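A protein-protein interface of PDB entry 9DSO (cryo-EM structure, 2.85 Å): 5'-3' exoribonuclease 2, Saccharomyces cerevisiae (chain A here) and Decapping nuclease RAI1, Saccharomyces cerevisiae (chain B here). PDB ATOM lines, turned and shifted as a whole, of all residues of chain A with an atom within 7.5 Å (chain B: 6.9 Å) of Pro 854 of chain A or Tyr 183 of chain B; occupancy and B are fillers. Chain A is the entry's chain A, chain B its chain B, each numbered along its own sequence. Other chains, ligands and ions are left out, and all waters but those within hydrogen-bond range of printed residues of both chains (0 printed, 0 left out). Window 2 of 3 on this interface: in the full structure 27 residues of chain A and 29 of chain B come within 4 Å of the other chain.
The backbone carbonyl oxygen (O) of Asn 179 of chain B lies within hydrogen-bond range of the side-chain hydroxyl (OG1) of Thr 184 of chain B, at 3.2 Å.
O of Pro 180 of chain B is in hydrogen-bond range of OG1 of Thr 184 of chain B, at 2.9 Å.
Among the printed residues, pairs that only touch across the chains: Ala 217 of chain A with Gln 182 of chain B, Pro 219 of chain A with Gln 182 of chain B and Pro 854 of chain A with Tyr 183 of chain B.
The side-chain hydroxyl (OG) of Ser 855 of chain A is in hydrogen-bond range of the backbone carbonyl oxygen (O) of Gln 182 of chain B, at 3.1 Å.
The side-chain amino group (NZ) of Lys 858 of chain A lies within hydrogen-bond range of the backbone carbonyl oxygen (O) of Leu 181 of chain B (2.8 Å).
The backbone carbonyl oxygen (O) of Thr 184 of chain B lies within hydrogen-bond range of the side-chain amino group (NZ) of Lys 858 of chain A (2.6 Å).
Printed residues of chain B within 4 Å of Pro 219 of chain A: Gln 182.
Of chain B, only Tyr 183 comes within 4 Å of Pro 854 of chain A.
Of the printed residues of chain A, Leu 181 of chain B touches Lys 858.
Of chain A, only Pro 854 (3.5 Å) comes within 4 Å of Tyr 183 of chain B.
Of the printed residues of chain A, Thr 184 of chain B touches Lys 858 (2.6 Å).
The nearest residue of chain A that does not touch Tyr 183 of chain B is Ser 855 of chain A (4.3 Å).
Of the 15 printed residues of chain A, 5 touch a printed residue of chain B.
Printed residues of chain A that touch a printed residue of chain B: Ala 217, Pro 219, Pro 854, Ser 855 and Lys 858.
Of the 7 printed residues of chain B, 4 touch a printed residue of chain A.
Hydrophobic or aromatic side chains of chain B that line the printed part of chain A: Tyr 183.
Among the printed residues, 6 pairs touch across the chains.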
ATOM      1  N   ARG A 213       9.762  34.852 -10.639  1.00  0.00           N
ATOM      2  CA  ARG A 213      10.074  33.629 -11.370  1.00  0.00           C
ATOM      3  C   ARG A 213       8.996  32.576 -11.170  1.00  0.00           C
ATOM      4  O   ARG A 213       8.594  31.903 -12.124  1.00  0.00           O
ATOM      5  CB  ARG A 213      11.431  33.088 -10.928  1.00  0.00           C
ATOM      6  CG  ARG A 213      12.591  33.537 -11.784  1.00  0.00           C
ATOM      7  CD  ARG A 213      13.837  32.739 -11.464  1.00  0.00           C
ATOM      8  NE  ARG A 213      14.425  33.115 -10.184  1.00  0.00           N
ATOM      9  CZ  ARG A 213      15.174  34.190  -9.991  1.00  0.00           C
ATOM     10  NH1 ARG A 213      15.430  35.038 -10.971  1.00  0.00           N
ATOM     11  NH2 ARG A 213      15.684  34.418  -8.784  1.00  0.00           N
ATOM     12  N   SER A 214       8.520  32.410  -9.935  1.00  0.00           N
ATOM     13  CA  SER A 214       7.445  31.449  -9.703  1.00  0.00           C
ATOM     14  C   SER A 214       6.147  31.883 -10.367  1.00  0.00           C
ATOM     15  O   SER A 214       5.349  31.034 -10.775  1.00  0.00           O
ATOM     16  CB  SER A 214       7.228  31.240  -8.209  1.00  0.00           C
ATOM     17  OG  SER A 214       8.326  30.561  -7.633  1.00  0.00           O
ATOM     18  N   ALA A 217       6.156  30.891 -14.174  1.00  0.00           N
ATOM     19  CA  ALA A 217       6.091  29.469 -14.488  1.00  0.00           C
ATOM     20  C   ALA A 217       4.670  28.933 -14.553  1.00  0.00           C
ATOM     21  O   ALA A 217       4.482  27.783 -14.962  1.00  0.00           O
ATOM     22  CB  ALA A 217       6.891  28.673 -13.461  1.00  0.00           C
ATOM     23  N   ASP A 218       3.684  29.709 -14.140  1.00  0.00           N
ATOM     24  CA  ASP A 218       2.297  29.288 -14.258  1.00  0.00           C
ATOM     25  C   ASP A 218       1.856  29.356 -15.715  1.00  0.00           C
ATOM     26  O   ASP A 218       2.088  30.373 -16.379  1.00  0.00           O
ATOM     27  CB  ASP A 218       1.406  30.177 -13.394  1.00  0.00           C
ATOM     28  CG  ASP A 218       0.116  29.501 -12.993  1.00  0.00           C
ATOM     29  OD1 ASP A 218      -0.015  28.281 -13.203  1.00  0.00           O
ATOM     30  OD2 ASP A 218      -0.777  30.192 -12.467  1.00  0.00           O
ATOM     31  N   PRO A 219       1.252  28.297 -16.259  1.00  0.00           N
ATOM     32  CA  PRO A 219       0.640  28.415 -17.591  1.00  0.00           C
ATOM     33  C   PRO A 219      -0.474  29.445 -17.651  1.00  0.00           C
ATOM     34  O   PRO A 219      -0.680  30.060 -18.704  1.00  0.00           O
ATOM     35  CB  PRO A 219       0.118  26.999 -17.861  1.00  0.00           C
ATOM     36  CG  PRO A 219       0.929  26.121 -16.988  1.00  0.00           C
ATOM     37  CD  PRO A 219       1.202  26.915 -15.756  1.00  0.00           C
ATOM     38  N   LYS A 801      -3.134  24.711  -3.538  1.00  0.00           N
ATOM     39  CA  LYS A 801      -2.326  25.326  -4.578  1.00  0.00           C
ATOM     40  C   LYS A 801      -3.268  25.958  -5.588  1.00  0.00           C
ATOM     41  O   LYS A 801      -4.122  25.272  -6.159  1.00  0.00           O
ATOM     42  CB  LYS A 801      -1.418  24.293  -5.242  1.00  0.00           C
ATOM     43  CG  LYS A 801      -0.965  24.661  -6.636  1.00  0.00           C
ATOM     44  CD  LYS A 801      -0.148  23.544  -7.255  1.00  0.00           C
ATOM     45  CE  LYS A 801      -0.113  23.661  -8.765  1.00  0.00           C
ATOM     46  NZ  LYS A 801       0.344  22.402  -9.410  1.00  0.00           N
ATOM     47  N   GLN A 803      -3.835  28.979  -8.878  1.00  0.00           N
ATOM     48  CA  GLN A 803      -3.163  29.454 -10.075  1.00  0.00           C
ATOM     49  C   GLN A 803      -3.679  30.834 -10.465  1.00  0.00           C
ATOM     50  O   GLN A 803      -4.555  31.406  -9.817  1.00  0.00           O
ATOM     51  CB  GLN A 803      -3.321  28.442 -11.210  1.00  0.00           C
ATOM     52  CG  GLN A 803      -2.406  27.246 -11.043  1.00  0.00           C
ATOM     53  CD  GLN A 803      -2.751  26.110 -11.967  1.00  0.00           C
ATOM     54  OE1 GLN A 803      -2.407  26.128 -13.147  1.00  0.00           O
ATOM     55  NE2 GLN A 803      -3.435  25.105 -11.435  1.00  0.00           N
ATOM     56  N   ILE A 851       5.071  28.136  -5.656  1.00  0.00           N
ATOM     57  CA  ILE A 851       5.044  26.858  -6.359  1.00  0.00           C
ATOM     58  C   ILE A 851       6.438  26.604  -6.918  1.00  0.00           C
ATOM     59  O   ILE A 851       6.971  27.452  -7.649  1.00  0.00           O
ATOM     60  CB  ILE A 851       3.985  26.846  -7.471  1.00  0.00           C
ATOM     61  CG1 ILE A 851       2.580  26.829  -6.878  1.00  0.00           C
ATOM     62  CG2 ILE A 851       4.178  25.645  -8.367  1.00  0.00           C
ATOM     63  CD1 ILE A 851       1.493  27.029  -7.902  1.00  0.00           C
ATOM     64  N   PRO A 852       7.066  25.472  -6.600  1.00  0.00           N
ATOM     65  CA  PRO A 852       8.425  25.220  -7.091  1.00  0.00           C
ATOM     66  C   PRO A 852       8.467  25.202  -8.609  1.00  0.00           C
ATOM     67  O   PRO A 852       7.546  24.715  -9.267  1.00  0.00           O
ATOM     68  CB  PRO A 852       8.766  23.847  -6.504  1.00  0.00           C
ATOM     69  CG  PRO A 852       7.821  23.668  -5.362  1.00  0.00           C
ATOM     70  CD  PRO A 852       6.569  24.376  -5.754  1.00  0.00           C
ATOM     71  N   LEU A 853       9.546  25.737  -9.162  1.00  0.00           N
ATOM     72  CA  LEU A 853       9.683  25.814 -10.610  1.00  0.00           C
ATOM     73  C   LEU A 853       9.738  24.410 -11.189  1.00  0.00           C
ATOM     74  O   LEU A 853      10.593  23.616 -10.779  1.00  0.00           O
ATOM     75  CB  LEU A 853      10.935  26.593 -10.993  1.00  0.00           C
ATOM     76  CG  LEU A 853      10.966  28.087 -10.676  1.00  0.00           C
ATOM     77  CD1 LEU A 853      12.317  28.672 -11.033  1.00  0.00           C
ATOM     78  CD2 LEU A 853       9.874  28.810 -11.418  1.00  0.00           C
ATOM     79  N   PRO A 854       8.850  24.054 -12.120  1.00  0.00           N
ATOM     80  CA  PRO A 854       8.905  22.705 -12.699  1.00  0.00           C
ATOM     81  C   PRO A 854      10.194  22.435 -13.445  1.00  0.00           C
ATOM     82  O   PRO A 854      10.631  21.281 -13.522  1.00  0.00           O
ATOM     83  CB  PRO A 854       7.691  22.681 -13.636  1.00  0.00           C
ATOM     84  CG  PRO A 854       7.468  24.114 -13.985  1.00  0.00           C
ATOM     85  CD  PRO A 854       7.830  24.896 -12.764  1.00  0.00           C
ATOM     86  N   SER A 855      10.816  23.472 -13.998  1.00  0.00           N
ATOM     87  CA  SER A 855      12.049  23.338 -14.753  1.00  0.00           C
ATOM     88  C   SER A 855      12.791  24.667 -14.703  1.00  0.00           C
ATOM     89  O   SER A 855      12.302  25.652 -14.144  1.00  0.00           O
ATOM     90  CB  SER A 855      11.754  22.893 -16.188  1.00  0.00           C
ATOM     91  OG  SER A 855      10.944  23.838 -16.860  1.00  0.00           O
ATOM     92  N   ARG A 856      13.986  24.686 -15.286  1.00  0.00           N
ATOM     93  CA  ARG A 856      14.796  25.896 -15.310  1.00  0.00           C
ATOM     94  C   ARG A 856      14.045  27.033 -15.988  1.00  0.00           C
ATOM     95  O   ARG A 856      13.423  26.845 -17.036  1.00  0.00           O
ATOM     96  CB  ARG A 856      16.113  25.626 -16.037  1.00  0.00           C
ATOM     97  CG  ARG A 856      16.970  26.854 -16.256  1.00  0.00           C
ATOM     98  CD  ARG A 856      18.229  26.516 -17.034  1.00  0.00           C
ATOM     99  NE  ARG A 856      19.126  25.664 -16.264  1.00  0.00           N
ATOM    100  CZ  ARG A 856      20.001  26.111 -15.373  1.00  0.00           C
ATOM    101  NH1 ARG A 856      20.131  27.402 -15.122  1.00  0.00           N
ATOM    102  NH2 ARG A 856      20.765  25.241 -14.720  1.00  0.00           N
ATOM    103  N   ASN A 857      14.096  28.214 -15.379  1.00  0.00           N
ATOM    104  CA  ASN A 857      13.428  29.376 -15.945  1.00  0.00           C
ATOM    105  C   ASN A 857      14.144  29.822 -17.211  1.00  0.00           C
ATOM    106  O   ASN A 857      15.365  29.992 -17.218  1.00  0.00           O
ATOM    107  CB  ASN A 857      13.390  30.513 -14.926  1.00  0.00           C
ATOM    108  CG  ASN A 857      12.406  31.599 -15.300  1.00  0.00           C
ATOM    109  OD1 ASN A 857      11.196  31.381 -15.309  1.00  0.00           O
ATOM    110  ND2 ASN A 857      12.923  32.779 -15.610  1.00  0.00           N
ATOM    111  N   LYS A 858      13.384  30.016 -18.281  1.00  0.00           N
ATOM    112  CA  LYS A 858      13.935  30.417 -19.565  1.00  0.00           C
ATOM    113  C   LYS A 858      13.815  31.922 -19.736  1.00  0.00           C
ATOM    114  O   LYS A 858      12.782  32.516 -19.418  1.00  0.00           O
ATOM    115  CB  LYS A 858      13.223  29.707 -20.716  1.00  0.00           C
ATOM    116  CG  LYS A 858      13.621  28.260 -20.905  1.00  0.00           C
ATOM    117  CD  LYS A 858      12.749  27.602 -21.952  1.00  0.00           C
ATOM    118  CE  LYS A 858      11.285  27.691 -21.580  1.00  0.00           C
ATOM    119  NZ  LYS A 858      10.895  26.617 -20.638  1.00  0.00           N
ATOM    120  N   ASN B 179       4.871  20.311 -25.876  1.00  0.00           N
ATOM    121  CA  ASN B 179       4.625  20.432 -24.449  1.00  0.00           C
ATOM    122  C   ASN B 179       4.513  21.909 -24.112  1.00  0.00           C
ATOM    123  O   ASN B 179       4.958  22.759 -24.889  1.00  0.00           O
ATOM    124  CB  ASN B 179       5.748  19.774 -23.637  1.00  0.00           C
ATOM    125  CG  ASN B 179       5.585  18.274 -23.531  1.00  0.00           C
ATOM    126  OD1 ASN B 179       4.681  17.785 -22.859  1.00  0.00           O
ATOM    127  ND2 ASN B 179       6.461  17.536 -24.195  1.00  0.00           N
ATOM    128  N   PRO B 180       3.913  22.250 -22.969  1.00  0.00           N
ATOM    129  CA  PRO B 180       3.749  23.667 -22.629  1.00  0.00           C
ATOM    130  C   PRO B 180       5.087  24.383 -22.560  1.00  0.00           C
ATOM    131  O   PRO B 180       6.115  23.793 -22.226  1.00  0.00           O
ATOM    132  CB  PRO B 180       3.067  23.626 -21.259  1.00  0.00           C
ATOM    133  CG  PRO B 180       2.370  22.333 -21.231  1.00  0.00           C
ATOM    134  CD  PRO B 180       3.228  21.379 -21.997  1.00  0.00           C
ATOM    135  N   LEU B 181       5.064  25.670 -22.908  1.00  0.00           N
ATOM    136  CA  LEU B 181       6.292  26.459 -22.932  1.00  0.00           C
ATOM    137  C   LEU B 181       6.991  26.445 -21.581  1.00  0.00           C
ATOM    138  O   LEU B 181       8.224  26.486 -21.507  1.00  0.00           O
ATOM    139  CB  LEU B 181       5.977  27.891 -23.350  1.00  0.00           C
ATOM    140  CG  LEU B 181       7.179  28.822 -23.419  1.00  0.00           C
ATOM    141  CD1 LEU B 181       8.144  28.345 -24.487  1.00  0.00           C
ATOM    142  CD2 LEU B 181       6.720  30.239 -23.677  1.00  0.00           C
ATOM    143  N   GLN B 182       6.218  26.389 -20.500  1.00  0.00           N
ATOM    144  CA  GLN B 182       6.789  26.344 -19.163  1.00  0.00           C
ATOM    145  C   GLN B 182       7.437  25.001 -18.858  1.00  0.00           C
ATOM    146  O   GLN B 182       8.174  24.892 -17.874  1.00  0.00           O
ATOM    147  CB  GLN B 182       5.701  26.657 -18.135  1.00  0.00           C
ATOM    148  CG  GLN B 182       5.070  28.030 -18.305  1.00  0.00           C
ATOM    149  CD  GLN B 182       3.991  28.065 -19.373  1.00  0.00           C
ATOM    150  OE1 GLN B 182       3.223  27.122 -19.522  1.00  0.00           O
ATOM    151  NE2 GLN B 182       3.930  29.161 -20.114  1.00  0.00           N
ATOM    152  N   TYR B 183       7.176  23.979 -19.672  1.00  0.00           N
ATOM    153  CA  TYR B 183       7.734  22.648 -19.473  1.00  0.00           C
ATOM    154  C   TYR B 183       8.709  22.252 -20.573  1.00  0.00           C
ATOM    155  O   TYR B 183       9.132  21.093 -20.624  1.00  0.00           O
ATOM    156  CB  TYR B 183       6.613  21.612 -19.385  1.00  0.00           C
ATOM    157  CG  TYR B 183       5.620  21.852 -18.274  1.00  0.00           C
ATOM    158  CD1 TYR B 183       5.960  22.600 -17.159  1.00  0.00           C
ATOM    159  CD2 TYR B 183       4.339  21.333 -18.344  1.00  0.00           C
ATOM    160  CE1 TYR B 183       5.056  22.824 -16.149  1.00  0.00           C
ATOM    161  CE2 TYR B 183       3.426  21.552 -17.336  1.00  0.00           C
ATOM    162  CZ  TYR B 183       3.790  22.300 -16.239  1.00  0.00           C
ATOM    163  OH  TYR B 183       2.888  22.522 -15.227  1.00  0.00           O
ATOM    164  N   THR B 184       9.076  23.180 -21.454  1.00  0.00           N
ATOM    165  CA  THR B 184       9.920  22.866 -22.594  1.00  0.00           C
ATOM    166  C   THR B 184      11.329  23.374 -22.348  1.00  0.00           C
ATOM    167  O   THR B 184      11.499  24.565 -22.047  1.00  0.00           O
ATOM    168  CB  THR B 184       9.353  23.487 -23.866  1.00  0.00           C
ATOM    169  OG1 THR B 184       8.086  22.896 -24.165  1.00  0.00           O
ATOM    170  CG2 THR B 184      10.286  23.255 -25.030  1.00  0.00           C
ATOM    171  N   PRO B 185      12.355  22.534 -22.452  1.00  0.00           N
ATOM    172  CA  PRO B 185      13.730  23.033 -22.371  1.00  0.00           C
ATOM    173  C   PRO B 185      14.070  23.918 -23.560  1.00  0.00           C
ATOM    174  O   PRO B 185      13.432  23.870 -24.612  1.00  0.00           O
ATOM    175  CB  PRO B 185      14.575  21.755 -22.373  1.00  0.00           C
ATOM    176  CG  PRO B 185      13.639  20.671 -21.989  1.00  0.00           C
ATOM    177  CD  PRO B 185      12.312  21.067 -22.532  1.00  0.00           C
